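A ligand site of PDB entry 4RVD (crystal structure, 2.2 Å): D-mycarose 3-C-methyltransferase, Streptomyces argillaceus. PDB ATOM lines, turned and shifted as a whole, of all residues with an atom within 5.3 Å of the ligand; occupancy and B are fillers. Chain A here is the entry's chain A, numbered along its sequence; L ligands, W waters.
Water W3 lies within hydrogen-bond range of the side-chain carboxylate (OE1) of Glu 112 (2.6 Å), the guanidinium group (NH1) of Arg 177 (3.0 Å) and a nitrogen (N1) of the ligand (3.2 Å).
The backbone NH (N) of Asn 116 sits at hydrogen-bond distance from the side-chain carboxylate (OD1) of Asp 135, at 2.9 Å. The backbone NH (N) of Ala 137 is in hydrogen-bond range of the side-chain carboxylate (OD2) of Asp 135. The backbone carbonyl oxygen (O) of Asp 135 lies within hydrogen-bond range of the backbone NH (N) of Glu 154 (3.5 Å). N of Gly 114 sits at hydrogen-bond distance from O of Ile 134 (2.7 Å). The backbone carbonyl oxygen (O) of His 178 lies close to a ring nitrogen (ND1) of His 182 (3.4 Å). The side-chain hydroxyl (OH) of Tyr 74 lies close to the backbone carbonyl oxygen (O) of Glu 225 (3.5 Å). OE1 of Glu 225 lies within hydrogen-bond range of OH of Tyr 77, 2.6 Å away. The backbone NH (N) of Ile 134 sits at hydrogen-bond distance from the side-chain hydroxyl (OG) of Ser 115, 3.4 Å away.
The side-chain carboxylate (OD1) of Asp 135 lies within hydrogen-bond range of an oxygen (O4) of the ligand (2.6 Å). The backbone carbonyl oxygen (O) of Arg 177 lies within hydrogen-bond range of a nitrogen (N1) of the ligand (2.8 Å). NH1 of Arg 177 lies within salt-bridge range of O1 of the ligand (3.0 Å). The side-chain amide nitrogen (ND2) of Asn 116 sits at hydrogen-bond distance from an oxygen (O4) of the ligand. The backbone NH of Gly 114 lies within hydrogen-bond range of a nitrogen (N6) of the ligand. N1 of the ligand lies within hydrogen-bond range of O of Gly 114 (2.9 Å). N5 of the ligand is in hydrogen-bond range of N of Phe 156.
A sulfur (S1) of the ligand lies close to the backbone carbonyl oxygen of His 178, 3.7 Å away. Merely in contact with the ligand: Pro 136 (3.2 Å), Ile 113 (3.4 Å), Val 179 (3.4 Å), Phe 155 (3.5 Å), Ile 183 (3.5 Å), Tyr 74 (3.7 Å), Ala 137 (3.7 Å), Tyr 77 (3.7 Å), His 182 (3.8 Å) and Ile 134 (3.9 Å). Hydrophobic or aromatic side chains within 4 Å of the ligand: Tyr 74, Ile 113, Pro 136, Ala 137, Phe 155, Phe 156, His 178, Val 179 and Ile 183. Of the 22 residues printed, 16 come within 4 Å of the ligand. The nearest printed residue that does not touch the ligand is Glu 112 (4.3 Å).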
ATOM      1  N   TYR A  74     -24.465 -20.760  -9.683  1.00  0.00           N
ATOM      2  CA  TYR A  74     -25.369 -21.495  -8.768  1.00  0.00           C
ATOM      3  C   TYR A  74     -26.434 -22.404  -9.398  1.00  0.00           C
ATOM      4  O   TYR A  74     -26.996 -23.249  -8.706  1.00  0.00           O
ATOM      5  CB  TYR A  74     -26.015 -20.499  -7.804  1.00  0.00           C
ATOM      6  CG  TYR A  74     -24.975 -19.753  -7.014  1.00  0.00           C
ATOM      7  CD1 TYR A  74     -24.037 -20.440  -6.250  1.00  0.00           C
ATOM      8  CD2 TYR A  74     -24.890 -18.359  -7.052  1.00  0.00           C
ATOM      9  CE1 TYR A  74     -23.062 -19.775  -5.546  1.00  0.00           C
ATOM     10  CE2 TYR A  74     -23.908 -17.686  -6.339  1.00  0.00           C
ATOM     11  CZ  TYR A  74     -22.991 -18.400  -5.588  1.00  0.00           C
ATOM     12  OH  TYR A  74     -21.996 -17.761  -4.879  1.00  0.00           O
ATOM     13  N   TYR A  77     -24.816 -26.766  -9.079  1.00  0.00           N
ATOM     14  CA  TYR A  77     -23.839 -26.594  -8.002  1.00  0.00           C
ATOM     15  C   TYR A  77     -23.415 -27.956  -7.430  1.00  0.00           C
ATOM     16  O   TYR A  77     -24.223 -28.877  -7.362  1.00  0.00           O
ATOM     17  CB  TYR A  77     -24.470 -25.698  -6.922  1.00  0.00           C
ATOM     18  CG  TYR A  77     -23.482 -25.043  -5.976  1.00  0.00           C
ATOM     19  CD1 TYR A  77     -22.592 -24.081  -6.429  1.00  0.00           C
ATOM     20  CD2 TYR A  77     -23.460 -25.375  -4.614  1.00  0.00           C
ATOM     21  CE1 TYR A  77     -21.689 -23.482  -5.573  1.00  0.00           C
ATOM     22  CE2 TYR A  77     -22.565 -24.784  -3.745  1.00  0.00           C
ATOM     23  CZ  TYR A  77     -21.680 -23.837  -4.225  1.00  0.00           C
ATOM     24  OH  TYR A  77     -20.789 -23.233  -3.373  1.00  0.00           O
ATOM     25  N   MET A  91     -25.331 -27.908  12.818  1.00  0.00           N
ATOM     26  CA  MET A  91     -26.722 -27.670  12.426  1.00  0.00           C
ATOM     27  C   MET A  91     -27.680 -27.839  13.616  1.00  0.00           C
ATOM     28  O   MET A  91     -28.646 -27.089  13.733  1.00  0.00           O
ATOM     29  CB  MET A  91     -27.117 -28.564  11.262  1.00  0.00           C
ATOM     30  CG  MET A  91     -26.466 -28.176   9.938  1.00  0.00           C
ATOM     31  SD  MET A  91     -27.161 -29.092   8.563  1.00  0.00           S
ATOM     32  CE  MET A  91     -26.197 -28.513   7.173  1.00  0.00           C
ATOM     33  N   GLU A 112     -35.648 -20.913   5.061  1.00  0.00           N
ATOM     34  CA  GLU A 112     -34.196 -20.877   4.869  1.00  0.00           C
ATOM     35  C   GLU A 112     -33.783 -20.564   3.437  1.00  0.00           C
ATOM     36  O   GLU A 112     -34.202 -21.229   2.497  1.00  0.00           O
ATOM     37  CB  GLU A 112     -33.534 -22.188   5.303  1.00  0.00           C
ATOM     38  CG  GLU A 112     -32.016 -22.161   5.116  1.00  0.00           C
ATOM     39  CD  GLU A 112     -31.314 -23.408   5.639  1.00  0.00           C
ATOM     40  OE1 GLU A 112     -30.076 -23.350   5.823  1.00  0.00           O
ATOM     41  OE2 GLU A 112     -31.996 -24.440   5.860  1.00  0.00           O
ATOM     42  N   ILE A 113     -32.908 -19.565   3.310  1.00  0.00           N
ATOM     43  CA  ILE A 113     -32.314 -19.141   2.071  1.00  0.00           C
ATOM     44  C   ILE A 113     -30.997 -19.883   1.879  1.00  0.00           C
ATOM     45  O   ILE A 113     -30.162 -19.901   2.785  1.00  0.00           O
ATOM     46  CB  ILE A 113     -32.030 -17.625   2.124  1.00  0.00           C
ATOM     47  CG1 ILE A 113     -33.340 -16.842   2.298  1.00  0.00           C
ATOM     48  CG2 ILE A 113     -31.307 -17.143   0.881  1.00  0.00           C
ATOM     49  CD1 ILE A 113     -33.133 -15.380   2.664  1.00  0.00           C
ATOM     50  N   GLY A 114     -30.793 -20.466   0.701  1.00  0.00           N
ATOM     51  CA  GLY A 114     -29.588 -21.253   0.432  1.00  0.00           C
ATOM     52  C   GLY A 114     -29.656 -22.586   1.159  1.00  0.00           C
ATOM     53  O   GLY A 114     -28.630 -23.105   1.616  1.00  0.00           O
ATOM     54  N   SER A 115     -30.870 -23.139   1.219  1.00  0.00           N
ATOM     55  CA  SER A 115     -31.162 -24.331   2.008  1.00  0.00           C
ATOM     56  C   SER A 115     -30.482 -25.593   1.485  1.00  0.00           C
ATOM     57  O   SER A 115     -30.366 -26.594   2.214  1.00  0.00           O
ATOM     58  CB  SER A 115     -32.674 -24.547   2.105  1.00  0.00           C
ATOM     59  OG  SER A 115     -33.271 -24.618   0.815  1.00  0.00           O
ATOM     60  N   ASN A 116     -30.046 -25.572   0.226  1.00  0.00           N
ATOM     61  CA  ASN A 116     -29.186 -26.628  -0.304  1.00  0.00           C
ATOM     62  C   ASN A 116     -29.938 -27.981  -0.282  1.00  0.00           C
ATOM     63  O   ASN A 116     -31.107 -28.022  -0.662  1.00  0.00           O
ATOM     64  CB  ASN A 116     -27.847 -26.648   0.469  1.00  0.00           C
ATOM     65  CG  ASN A 116     -26.707 -27.282  -0.318  1.00  0.00           C
ATOM     66  OD1 ASN A 116     -26.406 -28.454  -0.135  1.00  0.00           O
ATOM     67  ND2 ASN A 116     -26.082 -26.489  -1.197  1.00  0.00           N
ATOM     68  N   ILE A 134     -35.398 -22.047  -0.006  1.00  0.00           N
ATOM     69  CA  ILE A 134     -35.200 -21.308  -1.250  1.00  0.00           C
ATOM     70  C   ILE A 134     -33.759 -21.553  -1.671  1.00  0.00           C
ATOM     71  O   ILE A 134     -32.838 -21.200  -0.933  1.00  0.00           O
ATOM     72  CB  ILE A 134     -35.381 -19.777  -1.064  1.00  0.00           C
ATOM     73  CG1 ILE A 134     -36.711 -19.433  -0.400  1.00  0.00           C
ATOM     74  CG2 ILE A 134     -35.247 -19.038  -2.397  1.00  0.00           C
ATOM     75  CD1 ILE A 134     -37.915 -19.912  -1.175  1.00  0.00           C
ATOM     76  N   ASP A 135     -33.568 -22.160  -2.841  1.00  0.00           N
ATOM     77  CA  ASP A 135     -32.222 -22.407  -3.379  1.00  0.00           C
ATOM     78  C   ASP A 135     -32.254 -22.556  -4.900  1.00  0.00           C
ATOM     79  O   ASP A 135     -32.989 -23.380  -5.421  1.00  0.00           O
ATOM     80  CB  ASP A 135     -31.604 -23.662  -2.744  1.00  0.00           C
ATOM     81  CG  ASP A 135     -30.088 -23.741  -2.949  1.00  0.00           C
ATOM     82  OD1 ASP A 135     -29.337 -23.763  -1.945  1.00  0.00           O
ATOM     83  OD2 ASP A 135     -29.647 -23.762  -4.111  1.00  0.00           O
ATOM     84  N   PRO A 136     -31.438 -21.764  -5.623  1.00  0.00           N
ATOM     85  CA  PRO A 136     -31.470 -21.770  -7.099  1.00  0.00           C
ATOM     86  C   PRO A 136     -30.821 -22.976  -7.765  1.00  0.00           C
ATOM     87  O   PRO A 136     -31.106 -23.227  -8.938  1.00  0.00           O
ATOM     88  CB  PRO A 136     -30.683 -20.508  -7.452  1.00  0.00           C
ATOM     89  CG  PRO A 136     -29.731 -20.326  -6.317  1.00  0.00           C
ATOM     90  CD  PRO A 136     -30.482 -20.761  -5.100  1.00  0.00           C
ATOM     91  N   ALA A 137     -29.962 -23.707  -7.050  1.00  0.00           N
ATOM     92  CA  ALA A 137     -29.335 -24.912  -7.608  1.00  0.00           C
ATOM     93  C   ALA A 137     -30.373 -25.984  -7.912  1.00  0.00           C
ATOM     94  O   ALA A 137     -30.842 -26.680  -7.005  1.00  0.00           O
ATOM     95  CB  ALA A 137     -28.275 -25.444  -6.660  1.00  0.00           C
ATOM     96  N   ILE A 140     -29.669 -29.603  -6.873  1.00  0.00           N
ATOM     97  CA  ILE A 140     -29.696 -29.777  -5.425  1.00  0.00           C
ATOM     98  C   ILE A 140     -31.116 -29.673  -4.901  1.00  0.00           C
ATOM     99  O   ILE A 140     -31.509 -30.459  -4.038  1.00  0.00           O
ATOM    100  CB  ILE A 140     -28.766 -28.765  -4.732  1.00  0.00           C
ATOM    101  CG1 ILE A 140     -27.302 -29.074  -5.087  1.00  0.00           C
ATOM    102  CG2 ILE A 140     -28.958 -28.815  -3.226  1.00  0.00           C
ATOM    103  CD1 ILE A 140     -26.315 -28.011  -4.654  1.00  0.00           C
ATOM    104  N   GLU A 154     -35.381 -21.264  -6.782  1.00  0.00           N
ATOM    105  CA  GLU A 154     -35.158 -19.889  -7.222  1.00  0.00           C
ATOM    106  C   GLU A 154     -34.144 -19.162  -6.338  1.00  0.00           C
ATOM    107  O   GLU A 154     -33.788 -19.639  -5.239  1.00  0.00           O
ATOM    108  CB  GLU A 154     -36.477 -19.110  -7.204  1.00  0.00           C
ATOM    109  CG  GLU A 154     -37.630 -19.755  -7.971  1.00  0.00           C
ATOM    110  CD  GLU A 154     -37.342 -19.933  -9.456  1.00  0.00           C
ATOM    111  OE1 GLU A 154     -36.347 -19.389  -9.965  1.00  0.00           O
ATOM    112  OE2 GLU A 154     -38.134 -20.630 -10.124  1.00  0.00           O
ATOM    113  N   PHE A 155     -33.686 -18.013  -6.832  1.00  0.00           N
ATOM    114  CA  PHE A 155     -32.908 -17.083  -6.029  1.00  0.00           C
ATOM    115  C   PHE A 155     -33.875 -16.371  -5.103  1.00  0.00           C
ATOM    116  O   PHE A 155     -35.061 -16.281  -5.401  1.00  0.00           O
ATOM    117  CB  PHE A 155     -32.183 -16.043  -6.916  1.00  0.00           C
ATOM    118  CG  PHE A 155     -31.101 -16.636  -7.765  1.00  0.00           C
ATOM    119  CD1 PHE A 155     -29.800 -16.722  -7.292  1.00  0.00           C
ATOM    120  CD2 PHE A 155     -31.378 -17.103  -9.038  1.00  0.00           C
ATOM    121  CE1 PHE A 155     -28.795 -17.282  -8.070  1.00  0.00           C
ATOM    122  CE2 PHE A 155     -30.386 -17.659  -9.821  1.00  0.00           C
ATOM    123  CZ  PHE A 155     -29.086 -17.740  -9.338  1.00  0.00           C
ATOM    124  N   PHE A 156     -33.386 -15.895  -3.963  1.00  0.00           N
ATOM    125  CA  PHE A 156     -34.224 -15.129  -3.072  1.00  0.00           C
ATOM    126  C   PHE A 156     -34.379 -13.742  -3.673  1.00  0.00           C
ATOM    127  O   PHE A 156     -33.420 -13.188  -4.227  1.00  0.00           O
ATOM    128  CB  PHE A 156     -33.599 -15.019  -1.683  1.00  0.00           C
ATOM    129  CG  PHE A 156     -34.458 -14.284  -0.702  1.00  0.00           C
ATOM    130  CD1 PHE A 156     -35.616 -14.875  -0.213  1.00  0.00           C
ATOM    131  CD2 PHE A 156     -34.127 -13.010  -0.284  1.00  0.00           C
ATOM    132  CE1 PHE A 156     -36.425 -14.213   0.687  1.00  0.00           C
ATOM    133  CE2 PHE A 156     -34.932 -12.332   0.621  1.00  0.00           C
ATOM    134  CZ  PHE A 156     -36.076 -12.931   1.106  1.00  0.00           C
ATOM    135  N   ARG A 177     -27.482 -19.426   5.891  1.00  0.00           N
ATOM    136  CA  ARG A 177     -26.175 -19.896   6.331  1.00  0.00           C
ATOM    137  C   ARG A 177     -25.215 -19.932   5.157  1.00  0.00           C
ATOM    138  O   ARG A 177     -25.425 -20.667   4.187  1.00  0.00           O
ATOM    139  CB  ARG A 177     -26.287 -21.283   6.963  1.00  0.00           C
ATOM    140  CG  ARG A 177     -27.051 -21.313   8.280  1.00  0.00           C
ATOM    141  CD  ARG A 177     -26.858 -22.634   9.025  1.00  0.00           C
ATOM    142  NE  ARG A 177     -25.430 -22.910   9.252  1.00  0.00           N
ATOM    143  CZ  ARG A 177     -24.699 -23.793   8.574  1.00  0.00           C
ATOM    144  NH1 ARG A 177     -25.228 -24.562   7.630  1.00  0.00           N
ATOM    145  NH2 ARG A 177     -23.397 -23.907   8.860  1.00  0.00           N
ATOM    146  N   HIS A 178     -24.148 -19.135   5.259  1.00  0.00           N
ATOM    147  CA  HIS A 178     -23.122 -19.094   4.229  1.00  0.00           C
ATOM    148  C   HIS A 178     -23.733 -18.898   2.846  1.00  0.00           C
ATOM    149  O   HIS A 178     -23.450 -19.638   1.900  1.00  0.00           O
ATOM    150  CB  HIS A 178     -22.236 -20.342   4.329  1.00  0.00           C
ATOM    151  CG  HIS A 178     -21.590 -20.458   5.681  1.00  0.00           C
ATOM    152  ND1 HIS A 178     -20.427 -19.807   6.001  1.00  0.00           N
ATOM    153  CD2 HIS A 178     -22.004 -21.077   6.808  1.00  0.00           C
ATOM    154  CE1 HIS A 178     -20.135 -20.031   7.262  1.00  0.00           C
ATOM    155  NE2 HIS A 178     -21.073 -20.811   7.778  1.00  0.00           N
ATOM    156  N   VAL A 179     -24.603 -17.892   2.773  1.00  0.00           N
ATOM    157  CA  VAL A 179     -25.205 -17.468   1.520  1.00  0.00           C
ATOM    158  C   VAL A 179     -25.278 -15.938   1.403  1.00  0.00           C
ATOM    159  O   VAL A 179     -25.204 -15.409   0.301  1.00  0.00           O
ATOM    160  CB  VAL A 179     -26.612 -18.097   1.325  1.00  0.00           C
ATOM    161  CG1 VAL A 179     -27.587 -17.622   2.393  1.00  0.00           C
ATOM    162  CG2 VAL A 179     -27.153 -17.779  -0.057  1.00  0.00           C
ATOM    163  N   HIS A 182     -22.668 -14.385  -0.522  1.00  0.00           N
ATOM    164  CA  HIS A 182     -22.695 -14.834  -1.915  1.00  0.00           C
ATOM    165  C   HIS A 182     -23.616 -13.992  -2.804  1.00  0.00           C
ATOM    166  O   HIS A 182     -23.693 -14.227  -4.004  1.00  0.00           O
ATOM    167  CB  HIS A 182     -23.170 -16.298  -2.005  1.00  0.00           C
ATOM    168  CG  HIS A 182     -22.244 -17.290  -1.358  1.00  0.00           C
ATOM    169  ND1 HIS A 182     -21.958 -17.273  -0.020  1.00  0.00           N
ATOM    170  CD2 HIS A 182     -21.570 -18.338  -1.880  1.00  0.00           C
ATOM    171  CE1 HIS A 182     -21.138 -18.265   0.273  1.00  0.00           C
ATOM    172  NE2 HIS A 182     -20.892 -18.933  -0.848  1.00  0.00           N
ATOM    173  N   ILE A 183     -24.318 -13.016  -2.220  1.00  0.00           N
ATOM    174  CA  ILE A 183     -25.350 -12.250  -2.948  1.00  0.00           C
ATOM    175  C   ILE A 183     -24.909 -10.807  -3.168  1.00  0.00           C
ATOM    176  O   ILE A 183     -24.520 -10.120  -2.211  1.00  0.00           O
ATOM    177  CB  ILE A 183     -26.682 -12.242  -2.175  1.00  0.00           C
ATOM    178  CG1 ILE A 183     -27.156 -13.683  -1.928  1.00  0.00           C
ATOM    179  CG2 ILE A 183     -27.743 -11.454  -2.930  1.00  0.00           C
ATOM    180  CD1 ILE A 183     -28.183 -13.806  -0.828  1.00  0.00           C
ATOM    181  N   GLU A 225     -17.263 -16.757  -5.602  1.00  0.00           N
ATOM    182  CA  GLU A 225     -18.570 -16.926  -4.976  1.00  0.00           C
ATOM    183  C   GLU A 225     -18.694 -15.988  -3.791  1.00  0.00           C
ATOM    184  O   GLU A 225     -19.766 -15.441  -3.532  1.00  0.00           O
ATOM    185  CB  GLU A 225     -18.780 -18.364  -4.505  1.00  0.00           C
ATOM    186  CG  GLU A 225     -18.810 -19.374  -5.629  1.00  0.00           C
ATOM    187  CD  GLU A 225     -19.029 -20.787  -5.149  1.00  0.00           C
ATOM    188  OE1 GLU A 225     -19.651 -20.967  -4.083  1.00  0.00           O
ATOM    189  OE2 GLU A 225     -18.599 -21.721  -5.868  1.00  0.00           O
HETATM  190  N1  LIG L   1     -26.429 -23.187   3.487  1.00  0.00           N
HETATM  191  C1  LIG L   1     -25.590 -24.333   3.140  1.00  0.00           C
HETATM  192  C2  LIG L   1     -24.444 -24.497   4.113  1.00  0.00           C
HETATM  193  O1  LIG L   1     -24.229 -23.632   4.990  1.00  0.00           O
HETATM  194  O2  LIG L   1     -23.728 -25.518   3.998  1.00  0.00           O
HETATM  195  C3  LIG L   1     -25.040 -24.187   1.720  1.00  0.00           C
HETATM  196  C4  LIG L   1     -24.251 -22.900   1.501  1.00  0.00           C
HETATM  197  S1  LIG L   1     -23.608 -22.801  -0.048  1.00  0.00           S
HETATM  198  C5  LIG L   1     -21.977 -22.451   0.093  1.00  0.00           C
HETATM  199  C6  LIG L   1     -24.374 -21.604  -0.939  1.00  0.00           C
HETATM  200  C7  LIG L   1     -25.803 -22.031  -1.299  1.00  0.00           C
HETATM  201  O3  LIG L   1     -26.643 -20.874  -1.493  1.00  0.00           O
HETATM  202  C8  LIG L   1     -25.926 -22.851  -2.583  1.00  0.00           C
HETATM  203  O4  LIG L   1     -26.781 -23.990  -2.377  1.00  0.00           O
HETATM  204  C9  LIG L   1     -26.515 -21.898  -3.609  1.00  0.00           C
HETATM  205  O5  LIG L   1     -27.316 -22.539  -4.594  1.00  0.00           O
HETATM  206  C10 LIG L   1     -27.354 -20.984  -2.730  1.00  0.00           C
HETATM  207  N2  LIG L   1     -27.560 -19.607  -3.225  1.00  0.00           N
HETATM  208  C11 LIG L   1     -26.681 -18.839  -3.902  1.00  0.00           C
HETATM  209  N3  LIG L   1     -27.220 -17.631  -4.144  1.00  0.00           N
HETATM  210  C12 LIG L   1     -28.441 -17.601  -3.607  1.00  0.00           C
HETATM  211  C13 LIG L   1     -29.530 -16.610  -3.511  1.00  0.00           C
HETATM  212  N4  LIG L   1     -29.366 -15.391  -4.068  1.00  0.00           N
HETATM  213  N5  LIG L   1     -30.669 -16.970  -2.868  1.00  0.00           N
HETATM  214  C14 LIG L   1     -30.806 -18.204  -2.334  1.00  0.00           C
HETATM  215  N6  LIG L   1     -29.840 -19.154  -2.380  1.00  0.00           N
HETATM  216  C15 LIG L   1     -28.658 -18.908  -2.997  1.00  0.00           C
HETATM  217  O   HOH W   1     -28.755 -21.477   4.602  1.00  0.00           O
HETATM  218  O   HOH W   2     -22.186 -25.731   0.165  1.00  0.00           O
HETATM  219  O   HOH W   3     -27.751 -24.564   6.030  1.00  0.00           O
